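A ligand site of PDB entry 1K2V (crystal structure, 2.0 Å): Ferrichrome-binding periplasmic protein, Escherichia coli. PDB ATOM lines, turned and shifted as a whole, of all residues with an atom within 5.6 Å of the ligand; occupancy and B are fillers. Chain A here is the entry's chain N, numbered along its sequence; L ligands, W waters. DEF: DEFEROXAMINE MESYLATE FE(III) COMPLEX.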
ATOM      1  N   GLU A  12      -4.602   2.027  16.380  1.00  0.00           N
ATOM      2  CA  GLU A  12      -3.816   3.260  16.375  1.00  0.00           C
ATOM      3  C   GLU A  12      -4.525   4.224  17.317  1.00  0.00           C
ATOM      4  O   GLU A  12      -5.728   4.098  17.553  1.00  0.00           O
ATOM      5  CB  GLU A  12      -3.726   3.833  14.964  1.00  0.00           C
ATOM      6  CG  GLU A  12      -2.429   4.580  14.683  1.00  0.00           C
ATOM      7  CD  GLU A  12      -2.363   5.933  15.360  1.00  0.00           C
ATOM      8  OE1 GLU A  12      -3.171   6.804  14.994  1.00  0.00           O
ATOM      9  OE2 GLU A  12      -1.519   6.130  16.261  1.00  0.00           O
ATOM     10  N   TRP A  13      -3.789   5.194  17.852  1.00  0.00           N
ATOM     11  CA  TRP A  13      -4.366   6.124  18.802  1.00  0.00           C
ATOM     12  C   TRP A  13      -5.362   7.150  18.291  1.00  0.00           C
ATOM     13  O   TRP A  13      -6.186   7.630  19.055  1.00  0.00           O
ATOM     14  CB  TRP A  13      -3.273   6.816  19.607  1.00  0.00           C
ATOM     15  CG  TRP A  13      -2.374   5.836  20.316  1.00  0.00           C
ATOM     16  CD1 TRP A  13      -2.685   4.564  20.705  1.00  0.00           C
ATOM     17  CD2 TRP A  13      -1.011   6.044  20.691  1.00  0.00           C
ATOM     18  NE1 TRP A  13      -1.602   3.974  21.302  1.00  0.00           N
ATOM     19  CE2 TRP A  13      -0.555   4.863  21.306  1.00  0.00           C
ATOM     20  CE3 TRP A  13      -0.126   7.130  20.566  1.00  0.00           C
ATOM     21  CZ2 TRP A  13       0.744   4.726  21.803  1.00  0.00           C
ATOM     22  CZ3 TRP A  13       1.163   6.997  21.056  1.00  0.00           C
ATOM     23  CH2 TRP A  13       1.589   5.796  21.660  1.00  0.00           C
ATOM     24  N   ASP A  31      -0.868  -0.818  22.067  1.00  0.00           N
ATOM     25  CA  ASP A  31       0.081  -0.094  22.897  1.00  0.00           C
ATOM     26  C   ASP A  31      -0.573   0.835  23.924  1.00  0.00           C
ATOM     27  O   ASP A  31      -0.413   2.058  23.867  1.00  0.00           O
ATOM     28  CB  ASP A  31       1.037   0.694  21.998  1.00  0.00           C
ATOM     29  CG  ASP A  31       2.265   1.165  22.730  1.00  0.00           C
ATOM     30  OD1 ASP A  31       3.124   1.796  22.081  1.00  0.00           O
ATOM     31  OD2 ASP A  31       2.370   0.897  23.953  1.00  0.00           O
ATOM     32  N   ASN A  34       2.187   3.086  25.998  1.00  0.00           N
ATOM     33  CA  ASN A  34       2.624   4.351  25.437  1.00  0.00           C
ATOM     34  C   ASN A  34       1.469   5.313  25.244  1.00  0.00           C
ATOM     35  O   ASN A  34       1.657   6.534  25.254  1.00  0.00           O
ATOM     36  CB  ASN A  34       3.374   4.123  24.123  1.00  0.00           C
ATOM     37  CG  ASN A  34       4.732   3.472  24.359  1.00  0.00           C
ATOM     38  OD1 ASN A  34       5.502   3.920  25.203  1.00  0.00           O
ATOM     39  ND2 ASN A  34       5.034   2.413  23.595  1.00  0.00           N
ATOM     40  N   TRP A  38       2.035   9.304  25.885  1.00  0.00           N
ATOM     41  CA  TRP A  38       1.936  10.343  24.861  1.00  0.00           C
ATOM     42  C   TRP A  38       0.564  10.980  24.666  1.00  0.00           C
ATOM     43  O   TRP A  38       0.471  12.152  24.307  1.00  0.00           O
ATOM     44  CB  TRP A  38       2.421   9.801  23.515  1.00  0.00           C
ATOM     45  CG  TRP A  38       3.824   9.330  23.527  1.00  0.00           C
ATOM     46  CD1 TRP A  38       4.303   8.138  23.997  1.00  0.00           C
ATOM     47  CD2 TRP A  38       4.957  10.031  22.992  1.00  0.00           C
ATOM     48  NE1 TRP A  38       5.656   8.050  23.783  1.00  0.00           N
ATOM     49  CE2 TRP A  38       6.089   9.197  23.170  1.00  0.00           C
ATOM     50  CE3 TRP A  38       5.131  11.284  22.383  1.00  0.00           C
ATOM     51  CZ2 TRP A  38       7.365   9.573  22.745  1.00  0.00           C
ATOM     52  CZ3 TRP A  38       6.406  11.659  21.957  1.00  0.00           C
ATOM     53  CH2 TRP A  38       7.504  10.803  22.146  1.00  0.00           C
ATOM     54  N   LEU A  53       2.137  -3.380  19.961  1.00  0.00           N
ATOM     55  CA  LEU A  53       2.545  -2.113  19.332  1.00  0.00           C
ATOM     56  C   LEU A  53       1.717  -1.839  18.078  1.00  0.00           C
ATOM     57  O   LEU A  53       1.382  -2.749  17.337  1.00  0.00           O
ATOM     58  CB  LEU A  53       4.034  -2.140  18.961  1.00  0.00           C
ATOM     59  CG  LEU A  53       5.075  -2.417  20.047  1.00  0.00           C
ATOM     60  CD1 LEU A  53       6.457  -2.163  19.464  1.00  0.00           C
ATOM     61  CD2 LEU A  53       4.853  -1.526  21.257  1.00  0.00           C
ATOM     62  N   ARG A  54       1.407  -0.568  17.848  1.00  0.00           N
ATOM     63  CA  ARG A  54       0.613  -0.185  16.690  1.00  0.00           C
ATOM     64  C   ARG A  54       1.227  -0.637  15.375  1.00  0.00           C
ATOM     65  O   ARG A  54       0.505  -0.974  14.435  1.00  0.00           O
ATOM     66  CB  ARG A  54       0.403   1.319  16.681  1.00  0.00           C
ATOM     67  CG  ARG A  54      -0.338   1.820  17.908  1.00  0.00           C
ATOM     68  CD  ARG A  54       0.463   2.862  18.617  1.00  0.00           C
ATOM     69  NE  ARG A  54       0.411   4.140  17.931  1.00  0.00           N
ATOM     70  CZ  ARG A  54       1.432   4.977  17.810  1.00  0.00           C
ATOM     71  NH1 ARG A  54       2.610   4.694  18.323  1.00  0.00           N
ATOM     72  NH2 ARG A  54       1.250   6.128  17.167  1.00  0.00           N
ATOM     73  N   THR A  55       2.553  -0.650  15.311  1.00  0.00           N
ATOM     74  CA  THR A  55       3.244  -1.071  14.094  1.00  0.00           C
ATOM     75  C   THR A  55       3.439  -2.587  14.019  1.00  0.00           C
ATOM     76  O   THR A  55       3.790  -3.124  12.972  1.00  0.00           O
ATOM     77  CB  THR A  55       4.620  -0.397  13.989  1.00  0.00           C
ATOM     78  OG1 THR A  55       5.370  -0.652  15.168  1.00  0.00           O
ATOM     79  CG2 THR A  55       4.441   1.111  13.807  1.00  0.00           C
ATOM     80  N   TYR A  76      -0.635   4.229   8.139  1.00  0.00           N
ATOM     81  CA  TYR A  76       0.171   3.975   9.329  1.00  0.00           C
ATOM     82  C   TYR A  76      -0.032   2.542   9.813  1.00  0.00           C
ATOM     83  O   TYR A  76      -1.131   1.995   9.740  1.00  0.00           O
ATOM     84  CB  TYR A  76      -0.224   4.954  10.436  1.00  0.00           C
ATOM     85  CG  TYR A  76       0.612   4.798  11.677  1.00  0.00           C
ATOM     86  CD1 TYR A  76       1.841   5.453  11.806  1.00  0.00           C
ATOM     87  CD2 TYR A  76       0.221   3.947  12.716  1.00  0.00           C
ATOM     88  CE1 TYR A  76       2.652   5.256  12.915  1.00  0.00           C
ATOM     89  CE2 TYR A  76       1.020   3.743  13.825  1.00  0.00           C
ATOM     90  CZ  TYR A  76       2.231   4.399  13.926  1.00  0.00           C
ATOM     91  OH  TYR A  76       3.040   4.193  15.033  1.00  0.00           O
ATOM     92  N   THR A 151       8.622  19.072  20.889  1.00  0.00           N
ATOM     93  CA  THR A 151       8.727  17.937  21.792  1.00  0.00           C
ATOM     94  C   THR A 151      10.079  17.324  21.472  1.00  0.00           C
ATOM     95  O   THR A 151      10.490  17.273  20.309  1.00  0.00           O
ATOM     96  CB  THR A 151       7.598  16.901  21.587  1.00  0.00           C
ATOM     97  OG1 THR A 151       7.619  15.997  22.703  1.00  0.00           O
ATOM     98  CG2 THR A 151       7.789  16.120  20.307  1.00  0.00           C
ATOM     99  N   ILE A 153      12.602  14.536  20.752  1.00  0.00           N
ATOM    100  CA  ILE A 153      12.645  13.162  20.270  1.00  0.00           C
ATOM    101  C   ILE A 153      13.777  12.468  21.042  1.00  0.00           C
ATOM    102  O   ILE A 153      13.602  11.388  21.591  1.00  0.00           O
ATOM    103  CB  ILE A 153      12.940  13.130  18.767  1.00  0.00           C
ATOM    104  CG1 ILE A 153      11.799  13.813  18.015  1.00  0.00           C
ATOM    105  CG2 ILE A 153      13.117  11.690  18.295  1.00  0.00           C
ATOM    106  CD1 ILE A 153      12.035  13.936  16.532  1.00  0.00           C
ATOM    107  N   LEU A 159      11.341  17.800  17.723  1.00  0.00           N
ATOM    108  CA  LEU A 159      10.272  17.698  16.764  1.00  0.00           C
ATOM    109  C   LEU A 159       9.555  19.035  16.869  1.00  0.00           C
ATOM    110  O   LEU A 159       9.315  19.536  17.970  1.00  0.00           O
ATOM    111  CB  LEU A 159       9.296  16.579  17.149  1.00  0.00           C
ATOM    112  CG  LEU A 159       8.773  15.575  16.114  1.00  0.00           C
ATOM    113  CD1 LEU A 159       7.317  15.287  16.450  1.00  0.00           C
ATOM    114  CD2 LEU A 159       8.880  16.101  14.697  1.00  0.00           C
ATOM    115  N   ASN A 185       6.176  17.077   7.625  1.00  0.00           N
ATOM    116  CA  ASN A 185       5.768  15.839   6.990  1.00  0.00           C
ATOM    117  C   ASN A 185       4.249  15.954   6.907  1.00  0.00           C
ATOM    118  O   ASN A 185       3.671  16.986   7.295  1.00  0.00           O
ATOM    119  CB  ASN A 185       6.169  14.628   7.838  1.00  0.00           C
ATOM    120  CG  ASN A 185       5.701  14.750   9.281  1.00  0.00           C
ATOM    121  OD1 ASN A 185       4.618  15.265   9.546  1.00  0.00           O
ATOM    122  ND2 ASN A 185       6.519  14.276  10.212  1.00  0.00           N
ATOM    123  N   TRP A 187       2.008  14.563   8.636  1.00  0.00           N
ATOM    124  CA  TRP A 187       1.419  14.674   9.953  1.00  0.00           C
ATOM    125  C   TRP A 187       1.600  16.036  10.610  1.00  0.00           C
ATOM    126  O   TRP A 187       1.137  16.241  11.738  1.00  0.00           O
ATOM    127  CB  TRP A 187       1.966  13.557  10.850  1.00  0.00           C
ATOM    128  CG  TRP A 187       1.797  12.218  10.218  1.00  0.00           C
ATOM    129  CD1 TRP A 187       2.579  11.665   9.243  1.00  0.00           C
ATOM    130  CD2 TRP A 187       0.738  11.284  10.457  1.00  0.00           C
ATOM    131  NE1 TRP A 187       2.070  10.452   8.854  1.00  0.00           N
ATOM    132  CE2 TRP A 187       0.937  10.195   9.579  1.00  0.00           C
ATOM    133  CE3 TRP A 187      -0.367  11.268  11.323  1.00  0.00           C
ATOM    134  CZ2 TRP A 187       0.071   9.092   9.549  1.00  0.00           C
ATOM    135  CZ3 TRP A 187      -1.234  10.165  11.293  1.00  0.00           C
ATOM    136  CH2 TRP A 187      -1.001   9.090  10.401  1.00  0.00           C
ATOM    137  N   SER A 189       4.658  17.651  11.254  1.00  0.00           N
ATOM    138  CA  SER A 189       5.864  17.858  12.058  1.00  0.00           C
ATOM    139  C   SER A 189       7.131  17.570  11.271  1.00  0.00           C
ATOM    140  O   SER A 189       7.089  17.066  10.160  1.00  0.00           O
ATOM    141  CB  SER A 189       5.830  16.947  13.297  1.00  0.00           C
ATOM    142  OG  SER A 189       5.795  15.591  12.908  1.00  0.00           O
ATOM    143  N   TRP A 243      -1.304  14.465  22.482  1.00  0.00           N
ATOM    144  CA  TRP A 243      -1.057  13.706  21.271  1.00  0.00           C
ATOM    145  C   TRP A 243      -1.116  14.658  20.081  1.00  0.00           C
ATOM    146  O   TRP A 243      -2.121  15.312  19.842  1.00  0.00           O
ATOM    147  CB  TRP A 243      -2.064  12.581  21.093  1.00  0.00           C
ATOM    148  CG  TRP A 243      -1.681  11.612  20.012  1.00  0.00           C
ATOM    149  CD1 TRP A 243      -2.513  11.051  19.087  1.00  0.00           C
ATOM    150  CD2 TRP A 243      -0.371  11.097  19.757  1.00  0.00           C
ATOM    151  NE1 TRP A 243      -1.795  10.199  18.267  1.00  0.00           N
ATOM    152  CE2 TRP A 243      -0.481  10.218  18.655  1.00  0.00           C
ATOM    153  CE3 TRP A 243       0.883  11.287  20.348  1.00  0.00           C
ATOM    154  CZ2 TRP A 243       0.615   9.526  18.132  1.00  0.00           C
ATOM    155  CZ3 TRP A 243       1.982  10.605  19.826  1.00  0.00           C
ATOM    156  CH2 TRP A 243       1.834   9.736  18.734  1.00  0.00           C
ATOM    157  N   PHE A 244      -0.030  14.702  19.320  1.00  0.00           N
ATOM    158  CA  PHE A 244       0.050  15.611  18.176  1.00  0.00           C
ATOM    159  C   PHE A 244      -0.692  15.111  16.957  1.00  0.00           C
ATOM    160  O   PHE A 244      -0.993  15.881  16.059  1.00  0.00           O
ATOM    161  CB  PHE A 244       1.509  15.814  17.776  1.00  0.00           C
ATOM    162  CG  PHE A 244       2.480  15.425  18.836  1.00  0.00           C
ATOM    163  CD1 PHE A 244       3.310  14.334  18.658  1.00  0.00           C
ATOM    164  CD2 PHE A 244       2.594  16.172  20.008  1.00  0.00           C
ATOM    165  CE1 PHE A 244       4.244  13.975  19.628  1.00  0.00           C
ATOM    166  CE2 PHE A 244       3.514  15.825  20.994  1.00  0.00           C
ATOM    167  CZ  PHE A 244       4.344  14.717  20.790  1.00  0.00           C
ATOM    168  N   TYR A 245      -0.994  13.815  16.917  1.00  0.00           N
ATOM    169  CA  TYR A 245      -1.665  13.235  15.768  1.00  0.00           C
ATOM    170  C   TYR A 245      -3.049  12.694  16.077  1.00  0.00           C
ATOM    171  O   TYR A 245      -3.506  11.736  15.451  1.00  0.00           O
ATOM    172  CB  TYR A 245      -0.768  12.136  15.197  1.00  0.00           C
ATOM    173  CG  TYR A 245       0.653  12.605  15.030  1.00  0.00           C
ATOM    174  CD1 TYR A 245       1.716  11.888  15.599  1.00  0.00           C
ATOM    175  CD2 TYR A 245       0.950  13.773  14.323  1.00  0.00           C
ATOM    176  CE1 TYR A 245       3.036  12.310  15.460  1.00  0.00           C
ATOM    177  CE2 TYR A 245       2.274  14.216  14.179  1.00  0.00           C
ATOM    178  CZ  TYR A 245       3.309  13.476  14.747  1.00  0.00           C
ATOM    179  OH  TYR A 245       4.615  13.894  14.599  1.00  0.00           O
HETATM  180 FE   DEF L   1       4.826   7.536  15.747  1.00  0.00          FE
HETATM  181  O11 DEF L   1       6.739   7.404  15.268  1.00  0.00           O
HETATM  182  O12 DEF L   1       4.984   5.590  15.693  1.00  0.00           O
HETATM  183  O21 DEF L   1       4.716   7.416  17.712  1.00  0.00           O
HETATM  184  O22 DEF L   1       5.359   9.370  16.147  1.00  0.00           O
HETATM  185  O31 DEF L   1       4.902   8.511  14.065  1.00  0.00           O
HETATM  186  O32 DEF L   1       2.872   7.819  15.538  1.00  0.00           O
HETATM  187  N11 DEF L   1       7.082   6.090  15.176  1.00  0.00           N
HETATM  188  C11 DEF L   1       6.136   5.184  15.412  1.00  0.00           C
HETATM  189  C12 DEF L   1       6.418   3.629  15.342  1.00  0.00           C
HETATM  190  C13 DEF L   1       7.184   3.085  16.600  1.00  0.00           C
HETATM  191  C14 DEF L   1       6.355   3.104  17.916  1.00  0.00           C
HETATM  192  O13 DEF L   1       5.249   2.477  17.982  1.00  0.00           O
HETATM  193  N12 DEF L   1       6.851   3.794  19.012  1.00  0.00           N
HETATM  194  C15 DEF L   1       6.054   3.724  20.131  1.00  0.00           C
HETATM  195  C16 DEF L   1       5.091   4.959  20.183  1.00  0.00           C
HETATM  196  C18 DEF L   1       4.776   7.445  20.418  1.00  0.00           C
HETATM  197  C17 DEF L   1       5.824   6.307  20.386  1.00  0.00           C
HETATM  198  C19 DEF L   1       5.240   8.683  19.624  1.00  0.00           C
HETATM  199  N21 DEF L   1       5.166   8.541  18.257  1.00  0.00           N
HETATM  200  C21 DEF L   1       5.491   9.545  17.417  1.00  0.00           C
HETATM  201  C22 DEF L   1       5.968  10.909  18.062  1.00  0.00           C
HETATM  202  C23 DEF L   1       6.301  12.075  17.042  1.00  0.00           C
HETATM  203  C24 DEF L   1       7.188  11.663  15.833  1.00  0.00           C
HETATM  204  O23 DEF L   1       8.210  10.973  16.007  1.00  0.00           O
HETATM  205  N22 DEF L   1       6.812  12.069  14.571  1.00  0.00           N
HETATM  206  C25 DEF L   1       7.620  11.669  13.537  1.00  0.00           C
HETATM  207  C26 DEF L   1       6.758  11.558  12.231  1.00  0.00           C
HETATM  208  C27 DEF L   1       5.330  11.090  12.619  1.00  0.00           C
HETATM  209  C28 DEF L   1       4.813   9.888  11.815  1.00  0.00           C
HETATM  210  C29 DEF L   1       3.423   9.471  12.420  1.00  0.00           C
HETATM  211  N31 DEF L   1       3.624   8.791  13.622  1.00  0.00           N
HETATM  212  C31 DEF L   1       2.608   8.415  14.430  1.00  0.00           C
HETATM  213  C32 DEF L   1       1.138   8.723  14.000  1.00  0.00           C
HETATM  214  C39 DEF L   1       8.360   5.760  14.849  1.00  0.00           C
HETATM  215  O   HOH W   1       6.380   6.494  11.884  1.00  0.00           O
HETATM  216  O   HOH W   2       2.913   1.605  19.414  1.00  0.00           O
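The side-chain hydroxyl (OH) of Tyr 245 lies within hydrogen-bond range of a nitrogen (N22) of the ligand, 2.9 Å away. OH of Tyr 76 sits close to O12 of the ligand. An oxygen (O13) of the ligand sits close to the guanidinium group of Arg 54.
OD1 of Asn 185 is in hydrogen-bond range of N of Trp 187. The guanidinium group of Arg 54 lies within salt-bridge range of the side-chain carboxylate of Glu 12, 2.9 Å away. The side-chain hydroxyl (OH) of Tyr 76 sits close to the guanidinium group (NH1) of Arg 54 (3.4 Å). O of Asp 31 is in hydrogen-bond range of NE1 of Trp 13 (3.4 Å). OH of Tyr 245 is in hydrogen-bond range of OG of Ser 189. O of Trp 38 lies within hydrogen-bond range of N of Trp 243 (3.4 Å). ND2 of Asn 34 sits at hydrogen-bond distance from OD1 of Asp 31. O of Thr 151 lies within hydrogen-bond range of N of Leu 159, at 2.8 Å.
Merely in contact with the ligand: Trp 13 (3.7 Å), Asn 34 (3.8 Å), Trp 38 (3.5 Å), Thr 55 (3.6 Å), Leu 159 (3.4 Å), Asn 185 (3.4 Å), Trp 187 (3.8 Å), Trp 243 (3.6 Å) and Phe 244 (3.8 Å). Hydrophobic or aromatic side chains within 4 Å of the ligand: Trp 13, Trp 38, Tyr 76, Leu 159, Trp 187, Trp 243, Phe 244 and Tyr 245. The nearest printed residue that does not touch the ligand is Asp 31 (4.01 Å).
Water W2 lies within hydrogen-bond range of OD1 of Asp 31, O13 of the ligand and N of Arg 54.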
